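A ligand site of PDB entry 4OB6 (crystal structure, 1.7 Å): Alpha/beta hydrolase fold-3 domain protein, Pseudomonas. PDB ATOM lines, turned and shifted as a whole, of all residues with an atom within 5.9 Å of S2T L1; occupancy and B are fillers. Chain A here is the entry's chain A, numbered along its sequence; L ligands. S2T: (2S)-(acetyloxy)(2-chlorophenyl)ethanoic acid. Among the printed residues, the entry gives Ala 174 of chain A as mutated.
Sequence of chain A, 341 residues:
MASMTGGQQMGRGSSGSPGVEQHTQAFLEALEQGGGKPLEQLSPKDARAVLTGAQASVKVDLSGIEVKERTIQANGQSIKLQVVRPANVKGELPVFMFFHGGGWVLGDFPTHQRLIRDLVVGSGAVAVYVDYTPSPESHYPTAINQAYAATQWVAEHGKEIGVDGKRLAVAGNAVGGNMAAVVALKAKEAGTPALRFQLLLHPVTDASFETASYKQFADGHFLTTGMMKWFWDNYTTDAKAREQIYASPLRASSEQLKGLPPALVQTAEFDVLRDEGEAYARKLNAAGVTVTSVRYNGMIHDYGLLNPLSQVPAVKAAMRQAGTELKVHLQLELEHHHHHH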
ATOM      1  N   LEU A  39     -10.029 -21.632  15.738  1.00  0.00           N
ATOM      2  CA  LEU A  39      -9.374 -22.502  16.705  1.00  0.00           C
ATOM      3  C   LEU A  39     -10.380 -23.308  17.529  1.00  0.00           C
ATOM      4  O   LEU A  39     -10.187 -24.500  17.790  1.00  0.00           O
ATOM      5  CB  LEU A  39      -8.522 -21.635  17.632  1.00  0.00           C
ATOM      6  CG  LEU A  39      -7.483 -22.333  18.503  1.00  0.00           C
ATOM      7  CD1 LEU A  39      -6.420 -22.988  17.653  1.00  0.00           C
ATOM      8  CD2 LEU A  39      -6.858 -21.300  19.438  1.00  0.00           C
ATOM      9  N   LEU A  51      -0.806 -24.168  17.937  1.00  0.00           N
ATOM     10  CA  LEU A  51       0.124 -23.357  18.718  1.00  0.00           C
ATOM     11  C   LEU A  51       1.543 -23.888  18.603  1.00  0.00           C
ATOM     12  O   LEU A  51       2.484 -23.123  18.450  1.00  0.00           O
ATOM     13  CB  LEU A  51      -0.298 -23.325  20.197  1.00  0.00           C
ATOM     14  CG  LEU A  51       0.647 -22.597  21.147  1.00  0.00           C
ATOM     15  CD1 LEU A  51       0.775 -21.119  20.802  1.00  0.00           C
ATOM     16  CD2 LEU A  51       0.191 -22.784  22.608  1.00  0.00           C
ATOM     17  N   GLY A 101       0.069 -20.201  29.664  1.00  0.00           N
ATOM     18  CA  GLY A 101      -1.243 -19.897  29.131  1.00  0.00           C
ATOM     19  C   GLY A 101      -1.614 -20.844  28.002  1.00  0.00           C
ATOM     20  O   GLY A 101      -0.991 -21.904  27.816  1.00  0.00           O
ATOM     21  N   GLY A 102      -2.640 -20.464  27.257  1.00  0.00           N
ATOM     22  CA  GLY A 102      -3.201 -21.367  26.257  1.00  0.00           C
ATOM     23  C   GLY A 102      -4.658 -21.702  26.525  1.00  0.00           C
ATOM     24  O   GLY A 102      -5.177 -22.670  25.962  1.00  0.00           O
ATOM     25  N   GLY A 103      -5.322 -20.930  27.375  1.00  0.00           N
ATOM     26  CA  GLY A 103      -6.763 -21.111  27.558  1.00  0.00           C
ATOM     27  C   GLY A 103      -7.172 -22.418  28.224  1.00  0.00           C
ATOM     28  O   GLY A 103      -8.291 -22.903  28.013  1.00  0.00           O
ATOM     29  N   TRP A 104      -6.256 -22.963  29.024  1.00  0.00           N
ATOM     30  CA  TRP A 104      -6.378 -24.266  29.689  1.00  0.00           C
ATOM     31  C   TRP A 104      -6.335 -25.474  28.733  1.00  0.00           C
ATOM     32  O   TRP A 104      -5.828 -26.534  29.096  1.00  0.00           O
ATOM     33  CB  TRP A 104      -7.607 -24.342  30.621  1.00  0.00           C
ATOM     34  CG  TRP A 104      -7.592 -23.303  31.711  1.00  0.00           C
ATOM     35  CD1 TRP A 104      -6.764 -23.270  32.804  1.00  0.00           C
ATOM     36  CD2 TRP A 104      -8.468 -22.180  31.832  1.00  0.00           C
ATOM     37  NE1 TRP A 104      -7.070 -22.174  33.590  1.00  0.00           N
ATOM     38  CE2 TRP A 104      -8.109 -21.486  33.009  1.00  0.00           C
ATOM     39  CE3 TRP A 104      -9.519 -21.680  31.042  1.00  0.00           C
ATOM     40  CZ2 TRP A 104      -8.771 -20.325  33.421  1.00  0.00           C
ATOM     41  CZ3 TRP A 104     -10.163 -20.536  31.456  1.00  0.00           C
ATOM     42  CH2 TRP A 104      -9.795 -19.869  32.628  1.00  0.00           C
ATOM     43  N   LEU A 106      -4.828 -25.429  25.566  1.00  0.00           N
ATOM     44  CA  LEU A 106      -3.581 -25.443  24.808  1.00  0.00           C
ATOM     45  C   LEU A 106      -2.389 -25.128  25.692  1.00  0.00           C
ATOM     46  O   LEU A 106      -2.544 -24.777  26.869  1.00  0.00           O
ATOM     47  CB  LEU A 106      -3.632 -24.416  23.684  1.00  0.00           C
ATOM     48  CG  LEU A 106      -4.988 -24.182  23.026  1.00  0.00           C
ATOM     49  CD1 LEU A 106      -4.919 -23.072  22.002  1.00  0.00           C
ATOM     50  CD2 LEU A 106      -5.455 -25.460  22.390  1.00  0.00           C
ATOM     51  N   GLY A 107      -1.195 -25.219  25.110  1.00  0.00           N
ATOM     52  CA  GLY A 107       0.010 -24.799  25.796  1.00  0.00           C
ATOM     53  C   GLY A 107       0.702 -25.932  26.512  1.00  0.00           C
ATOM     54  O   GLY A 107       0.119 -26.972  26.811  1.00  0.00           O
ATOM     55  N   HIS A 112       6.010 -22.415  25.291  1.00  0.00           N
ATOM     56  CA  HIS A 112       6.267 -21.258  26.149  1.00  0.00           C
ATOM     57  C   HIS A 112       7.740 -21.060  26.476  1.00  0.00           C
ATOM     58  O   HIS A 112       8.076 -20.156  27.242  1.00  0.00           O
ATOM     59  CB  HIS A 112       5.470 -21.419  27.459  1.00  0.00           C
ATOM     60  CG  HIS A 112       4.022 -21.067  27.320  1.00  0.00           C
ATOM     61  ND1 HIS A 112       3.151 -21.799  26.540  1.00  0.00           N
ATOM     62  CD2 HIS A 112       3.299 -20.060  27.854  1.00  0.00           C
ATOM     63  CE1 HIS A 112       1.947 -21.258  26.610  1.00  0.00           C
ATOM     64  NE2 HIS A 112       2.008 -20.198  27.391  1.00  0.00           N
ATOM     65  N   ASN A 173       1.226 -16.119  31.998  1.00  0.00           N
ATOM     66  CA  ASN A 173       0.572 -15.354  30.936  1.00  0.00           C
ATOM     67  C   ASN A 173      -0.852 -15.851  30.693  1.00  0.00           C
ATOM     68  O   ASN A 173      -1.091 -17.058  30.591  1.00  0.00           O
ATOM     69  CB  ASN A 173       1.362 -15.466  29.626  1.00  0.00           C
ATOM     70  CG  ASN A 173       1.551 -16.910  29.167  1.00  0.00           C
ATOM     71  OD1 ASN A 173       2.085 -17.746  29.913  1.00  0.00           O
ATOM     72  ND2 ASN A 173       1.117 -17.206  27.941  1.00  0.00           N
ATOM     73  N   ALA A 174      -1.794 -14.913  30.616  1.00  0.00           N
ATOM     74  CA  ALA A 174      -3.186 -15.213  30.204  1.00  0.00           C
ATOM     75  C   ALA A 174      -3.878 -16.114  31.222  1.00  0.00           C
ATOM     76  O   ALA A 174      -4.009 -15.698  32.372  1.00  0.00           O
ATOM     77  CB  ALA A 174      -3.221 -15.776  28.785  1.00  0.00           C
ATOM     78  N   VAL A 175      -4.319 -17.331  30.871  1.00  0.00           N
ATOM     79  CA  VAL A 175      -4.833 -18.184  31.954  1.00  0.00           C
ATOM     80  C   VAL A 175      -3.739 -18.564  32.931  1.00  0.00           C
ATOM     81  O   VAL A 175      -4.017 -18.941  34.072  1.00  0.00           O
ATOM     82  CB  VAL A 175      -5.576 -19.458  31.480  1.00  0.00           C
ATOM     83  CG1 VAL A 175      -6.729 -19.095  30.580  1.00  0.00           C
ATOM     84  CG2 VAL A 175      -4.618 -20.433  30.807  1.00  0.00           C
ATOM     85  N   GLY A 176      -2.483 -18.440  32.498  1.00  0.00           N
ATOM     86  CA  GLY A 176      -1.382 -18.614  33.425  1.00  0.00           C
ATOM     87  C   GLY A 176      -1.293 -17.467  34.417  1.00  0.00           C
ATOM     88  O   GLY A 176      -0.848 -17.650  35.551  1.00  0.00           O
ATOM     89  N   VAL A 204      -6.359 -13.547  32.686  1.00  0.00           N
ATOM     90  CA  VAL A 204      -7.802 -13.785  32.710  1.00  0.00           C
ATOM     91  C   VAL A 204      -8.218 -13.642  34.164  1.00  0.00           C
ATOM     92  O   VAL A 204      -7.626 -14.275  35.031  1.00  0.00           O
ATOM     93  CB  VAL A 204      -8.086 -15.218  32.237  1.00  0.00           C
ATOM     94  CG1 VAL A 204      -9.543 -15.585  32.466  1.00  0.00           C
ATOM     95  CG2 VAL A 204      -7.714 -15.368  30.775  1.00  0.00           C
ATOM     96  N   PHE A 222      -6.340 -11.480  17.211  1.00  0.00           N
ATOM     97  CA  PHE A 222      -5.698 -12.727  17.646  1.00  0.00           C
ATOM     98  C   PHE A 222      -6.559 -13.533  18.626  1.00  0.00           C
ATOM     99  O   PHE A 222      -7.153 -14.536  18.217  1.00  0.00           O
ATOM    100  CB  PHE A 222      -4.277 -12.479  18.164  1.00  0.00           C
ATOM    101  CG  PHE A 222      -3.605 -13.720  18.672  1.00  0.00           C
ATOM    102  CD1 PHE A 222      -3.351 -14.786  17.822  1.00  0.00           C
ATOM    103  CD2 PHE A 222      -3.207 -13.807  19.997  1.00  0.00           C
ATOM    104  CE1 PHE A 222      -2.736 -15.934  18.294  1.00  0.00           C
ATOM    105  CE2 PHE A 222      -2.583 -14.945  20.474  1.00  0.00           C
ATOM    106  CZ  PHE A 222      -2.352 -16.011  19.623  1.00  0.00           C
ATOM    107  N   LEU A 223      -6.634 -13.101  19.878  1.00  0.00           N
ATOM    108  CA  LEU A 223      -7.533 -13.729  20.844  1.00  0.00           C
ATOM    109  C   LEU A 223      -8.937 -13.187  20.643  1.00  0.00           C
ATOM    110  O   LEU A 223      -9.140 -11.972  20.684  1.00  0.00           O
ATOM    111  CB  LEU A 223      -7.088 -13.442  22.281  1.00  0.00           C
ATOM    112  CG  LEU A 223      -8.038 -13.920  23.382  1.00  0.00           C
ATOM    113  CD1 LEU A 223      -8.098 -15.444  23.406  1.00  0.00           C
ATOM    114  CD2 LEU A 223      -7.612 -13.378  24.744  1.00  0.00           C
ATOM    115  N   THR A 224      -9.895 -14.077  20.423  1.00  0.00           N
ATOM    116  CA  THR A 224     -11.269 -13.659  20.168  1.00  0.00           C
ATOM    117  C   THR A 224     -12.173 -13.998  21.338  1.00  0.00           C
ATOM    118  O   THR A 224     -11.825 -14.815  22.196  1.00  0.00           O
ATOM    119  CB  THR A 224     -11.842 -14.366  18.925  1.00  0.00           C
ATOM    120  OG1 THR A 224     -11.968 -15.775  19.176  1.00  0.00           O
ATOM    121  CG2 THR A 224     -10.943 -14.128  17.720  1.00  0.00           C
ATOM    122  N   MET A 227     -12.992 -17.657  21.278  1.00  0.00           N
ATOM    123  CA  MET A 227     -11.974 -18.500  21.894  1.00  0.00           C
ATOM    124  C   MET A 227     -12.119 -18.472  23.405  1.00  0.00           C
ATOM    125  O   MET A 227     -12.065 -19.518  24.059  1.00  0.00           O
ATOM    126  CB  MET A 227     -10.572 -18.043  21.517  1.00  0.00           C
ATOM    127  CG  MET A 227     -10.202 -18.335  20.091  1.00  0.00           C
ATOM    128  SD  MET A 227      -8.771 -17.350  19.626  1.00  0.00           S
ATOM    129  CE  MET A 227      -8.828 -17.515  17.852  1.00  0.00           C
ATOM    130  N   MET A 228     -12.295 -17.280  23.963  1.00  0.00           N
ATOM    131  CA  MET A 228     -12.340 -17.150  25.418  1.00  0.00           C
ATOM    132  C   MET A 228     -13.517 -17.921  26.009  1.00  0.00           C
ATOM    133  O   MET A 228     -13.397 -18.537  27.063  1.00  0.00           O
ATOM    134  CB  MET A 228     -12.435 -15.685  25.849  1.00  0.00           C
ATOM    135  CG  MET A 228     -11.113 -14.932  25.849  1.00  0.00           C
ATOM    136  SD  MET A 228      -9.822 -15.745  26.826  1.00  0.00           S
ATOM    137  CE  MET A 228     -10.647 -16.024  28.384  1.00  0.00           C
ATOM    138  N   PHE A 231     -12.553 -21.607  25.795  1.00  0.00           N
ATOM    139  CA  PHE A 231     -11.576 -21.893  26.836  1.00  0.00           C
ATOM    140  C   PHE A 231     -12.271 -22.101  28.171  1.00  0.00           C
ATOM    141  O   PHE A 231     -12.051 -23.109  28.835  1.00  0.00           O
ATOM    142  CB  PHE A 231     -10.582 -20.734  26.957  1.00  0.00           C
ATOM    143  CG  PHE A 231      -9.627 -20.606  25.802  1.00  0.00           C
ATOM    144  CD1 PHE A 231      -9.298 -21.691  24.994  1.00  0.00           C
ATOM    145  CD2 PHE A 231      -9.028 -19.378  25.532  1.00  0.00           C
ATOM    146  CE1 PHE A 231      -8.389 -21.560  23.951  1.00  0.00           C
ATOM    147  CE2 PHE A 231      -8.115 -19.229  24.489  1.00  0.00           C
ATOM    148  CZ  PHE A 231      -7.804 -20.315  23.694  1.00  0.00           C
ATOM    149  N   LEU A 273      -9.110  -9.089  27.094  1.00  0.00           N
ATOM    150  CA  LEU A 273      -8.862  -9.221  28.530  1.00  0.00           C
ATOM    151  C   LEU A 273      -8.301  -7.962  29.195  1.00  0.00           C
ATOM    152  O   LEU A 273      -8.102  -7.937  30.403  1.00  0.00           O
ATOM    153  CB  LEU A 273      -7.863 -10.350  28.786  1.00  0.00           C
ATOM    154  CG  LEU A 273      -8.216 -11.719  28.198  1.00  0.00           C
ATOM    155  CD1 LEU A 273      -7.117 -12.682  28.514  1.00  0.00           C
ATOM    156  CD2 LEU A 273      -9.558 -12.235  28.738  1.00  0.00           C
ATOM    157  N   HIS A 301      -3.082  -9.094  22.611  1.00  0.00           N
ATOM    158  CA  HIS A 301      -3.034 -10.091  23.687  1.00  0.00           C
ATOM    159  C   HIS A 301      -1.785 -10.974  23.634  1.00  0.00           C
ATOM    160  O   HIS A 301      -1.460 -11.531  22.584  1.00  0.00           O
ATOM    161  CB  HIS A 301      -4.254 -11.006  23.600  1.00  0.00           C
ATOM    162  CG  HIS A 301      -4.210 -12.138  24.564  1.00  0.00           C
ATOM    163  ND1 HIS A 301      -4.401 -11.963  25.920  1.00  0.00           N
ATOM    164  CD2 HIS A 301      -3.975 -13.455  24.388  1.00  0.00           C
ATOM    165  CE1 HIS A 301      -4.280 -13.132  26.531  1.00  0.00           C
ATOM    166  NE2 HIS A 301      -4.019 -14.057  25.621  1.00  0.00           N
ATOM    167  N   ASP A 302      -1.130 -11.084  24.787  1.00  0.00           N
ATOM    168  CA  ASP A 302      -0.025 -12.021  25.006  1.00  0.00           C
ATOM    169  C   ASP A 302       1.116 -11.857  24.003  1.00  0.00           C
ATOM    170  O   ASP A 302       1.678 -12.843  23.514  1.00  0.00           O
ATOM    171  CB  ASP A 302      -0.545 -13.459  25.008  1.00  0.00           C
ATOM    172  CG  ASP A 302       0.172 -14.315  26.015  1.00  0.00           C
ATOM    173  OD1 ASP A 302       1.155 -13.853  26.640  1.00  0.00           O
ATOM    174  OD2 ASP A 302      -0.254 -15.469  26.176  1.00  0.00           O
ATOM    175  N   LEU A 305       4.173 -14.010  24.707  1.00  0.00           N
ATOM    176  CA  LEU A 305       4.214 -15.422  24.349  1.00  0.00           C
ATOM    177  C   LEU A 305       4.648 -15.589  22.888  1.00  0.00           C
ATOM    178  O   LEU A 305       5.503 -16.424  22.575  1.00  0.00           O
ATOM    179  CB  LEU A 305       2.836 -16.053  24.507  1.00  0.00           C
ATOM    180  CG  LEU A 305       2.732 -17.483  23.970  1.00  0.00           C
ATOM    181  CD1 LEU A 305       3.703 -18.423  24.714  1.00  0.00           C
ATOM    182  CD2 LEU A 305       1.302 -18.011  24.084  1.00  0.00           C
ATOM    183  N   LEU A 306       4.044 -14.779  22.020  1.00  0.00           N
ATOM    184  CA  LEU A 306       4.088 -15.016  20.574  1.00  0.00           C
ATOM    185  C   LEU A 306       5.491 -14.884  19.969  1.00  0.00           C
ATOM    186  O   LEU A 306       6.066 -13.805  19.920  1.00  0.00           O
ATOM    187  CB  LEU A 306       3.099 -14.095  19.857  1.00  0.00           C
ATOM    188  CG  LEU A 306       1.645 -14.253  20.290  1.00  0.00           C
ATOM    189  CD1 LEU A 306       0.764 -13.254  19.552  1.00  0.00           C
ATOM    190  CD2 LEU A 306       1.174 -15.670  20.034  1.00  0.00           C
HETATM  191  C10 S2T L   1      -5.276 -17.641  26.891  1.00  0.00           C
HETATM  192  C01 S2T L   1      -3.690 -19.026  21.348  1.00  0.00           C
HETATM  193  C02 S2T L   1      -4.725 -18.259  20.844  1.00  0.00           C
HETATM  194  C03 S2T L   1      -5.424 -17.424  21.694  1.00  0.00           C
HETATM  195  C04 S2T L   1      -5.088 -17.331  23.041  1.00  0.00           C
HETATM  196  C05 S2T L   1      -4.058 -18.095  23.569  1.00  0.00           C
HETATM  197  C06 S2T L   1      -3.363 -18.936  22.698  1.00  0.00           C
HETATM  198  C07 S2T L   1      -3.723 -17.980  25.053  1.00  0.00           C
HETATM  199  O08 S2T L   1      -4.607 -17.127  25.746  1.00  0.00           O
HETATM  200  C09 S2T L   1      -2.381 -17.314  25.160  1.00  0.00           C
HETATM  201  O11 S2T L   1      -4.720 -18.250  27.816  1.00  0.00           O
HETATM  202  C12 S2T L   1      -6.504 -16.850  27.274  1.00  0.00           C
HETATM  203 CL   S2T L   1      -2.045 -19.931  23.233  1.00  0.00          CL
HETATM  204  O14 S2T L   1      -1.563 -17.765  26.012  1.00  0.00           O
HETATM  205  O15 S2T L   1      -2.121 -16.340  24.387  1.00  0.00           O
HETATM  206  C10 S2T L   2      -4.679 -18.902  15.770  1.00  0.00           C
HETATM  207  C01 S2T L   2       0.395 -18.591  17.726  1.00  0.00           C
HETATM  208  C02 S2T L   2       1.300 -17.770  17.067  1.00  0.00           C
HETATM  209  C03 S2T L   2       0.982 -17.284  15.808  1.00  0.00           C
HETATM  210  C04 S2T L   2      -0.228 -17.610  15.227  1.00  0.00           C
HETATM  211  C05 S2T L   2      -1.142 -18.447  15.872  1.00  0.00           C
HETATM  212  C06 S2T L   2      -0.820 -18.934  17.145  1.00  0.00           C
HETATM  213  C07 S2T L   2      -2.461 -18.723  15.135  1.00  0.00           C
HETATM  214  O08 S2T L   2      -3.390 -19.444  15.918  1.00  0.00           O
HETATM  215  C09 S2T L   2      -2.325 -19.380  13.767  1.00  0.00           C
HETATM  216  O11 S2T L   2      -5.411 -19.298  14.878  1.00  0.00           O
HETATM  217  C12 S2T L   2      -5.270 -18.059  16.884  1.00  0.00           C
HETATM  218 CL   S2T L   2      -1.835 -19.985  18.114  1.00  0.00          CL
HETATM  219  O14 S2T L   2      -3.295 -19.311  12.963  1.00  0.00           O
HETATM  220  O15 S2T L   2      -1.278 -19.981  13.424  1.00  0.00           O
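An oxygen (O14) of S2T L1 sits close to the side-chain carboxylate (OD2) of Asp 302 (2.6 Å). The backbone NH (N) of Gly 103 sits at hydrogen-bond distance from an oxygen (O11) of S2T L1. The backbone NH (N) of Gly 102 sits at hydrogen-bond distance from an oxygen (O11) of S2T L1, at 3.1 Å. NE2 of His 301 lies within hydrogen-bond range of O08 of S2T L1, at 3.1 Å. N of Val 175 lies within hydrogen-bond range of O11 of S2T L1, at 3.2 Å. ND2 of Asn 173 is in hydrogen-bond range of O14 of S2T L1, at 3.3 Å.
The side-chain carboxylate of Asp 302 is in hydrogen-bond range of the side-chain amide nitrogen of Asn 173 (2.8 Å). The backbone carbonyl oxygen (O) of Ala 174 lies within hydrogen-bond range of the backbone NH (N) of Val 204 (3.2 Å). The backbone NH (N) of Gly 101 sits at hydrogen-bond distance from the side-chain amide oxygen (OD1) of Asn 173, at 3.2 Å. The side-chain amide nitrogen (ND2) of Asn 173 sits at hydrogen-bond distance from a ring nitrogen (NE2) of His 112 (3.2 Å). A ring nitrogen (NE2) of His 112 sits at hydrogen-bond distance from the backbone NH (N) of Gly 101 (3.0 Å). N of Met 227 sits at hydrogen-bond distance from OG1 of Thr 224, at 3.0 Å.
Merely in contact with S2T L1: Ala 174, Leu 305, Phe 222, Met 228, Leu 223, Gly 101, Leu 51, Phe 231, Met 227, Leu 39 and Val 204. Hydrophobic or aromatic side chains within 4 Å of S2T L1: Leu 39, Leu 51, Ala 174, Val 175, Val 204, Phe 222, Leu 223, Met 227, Met 228, Phe 231, His 301 and Leu 305. Of the 25 residues printed, 17 come within 4 Å of S2T L1.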
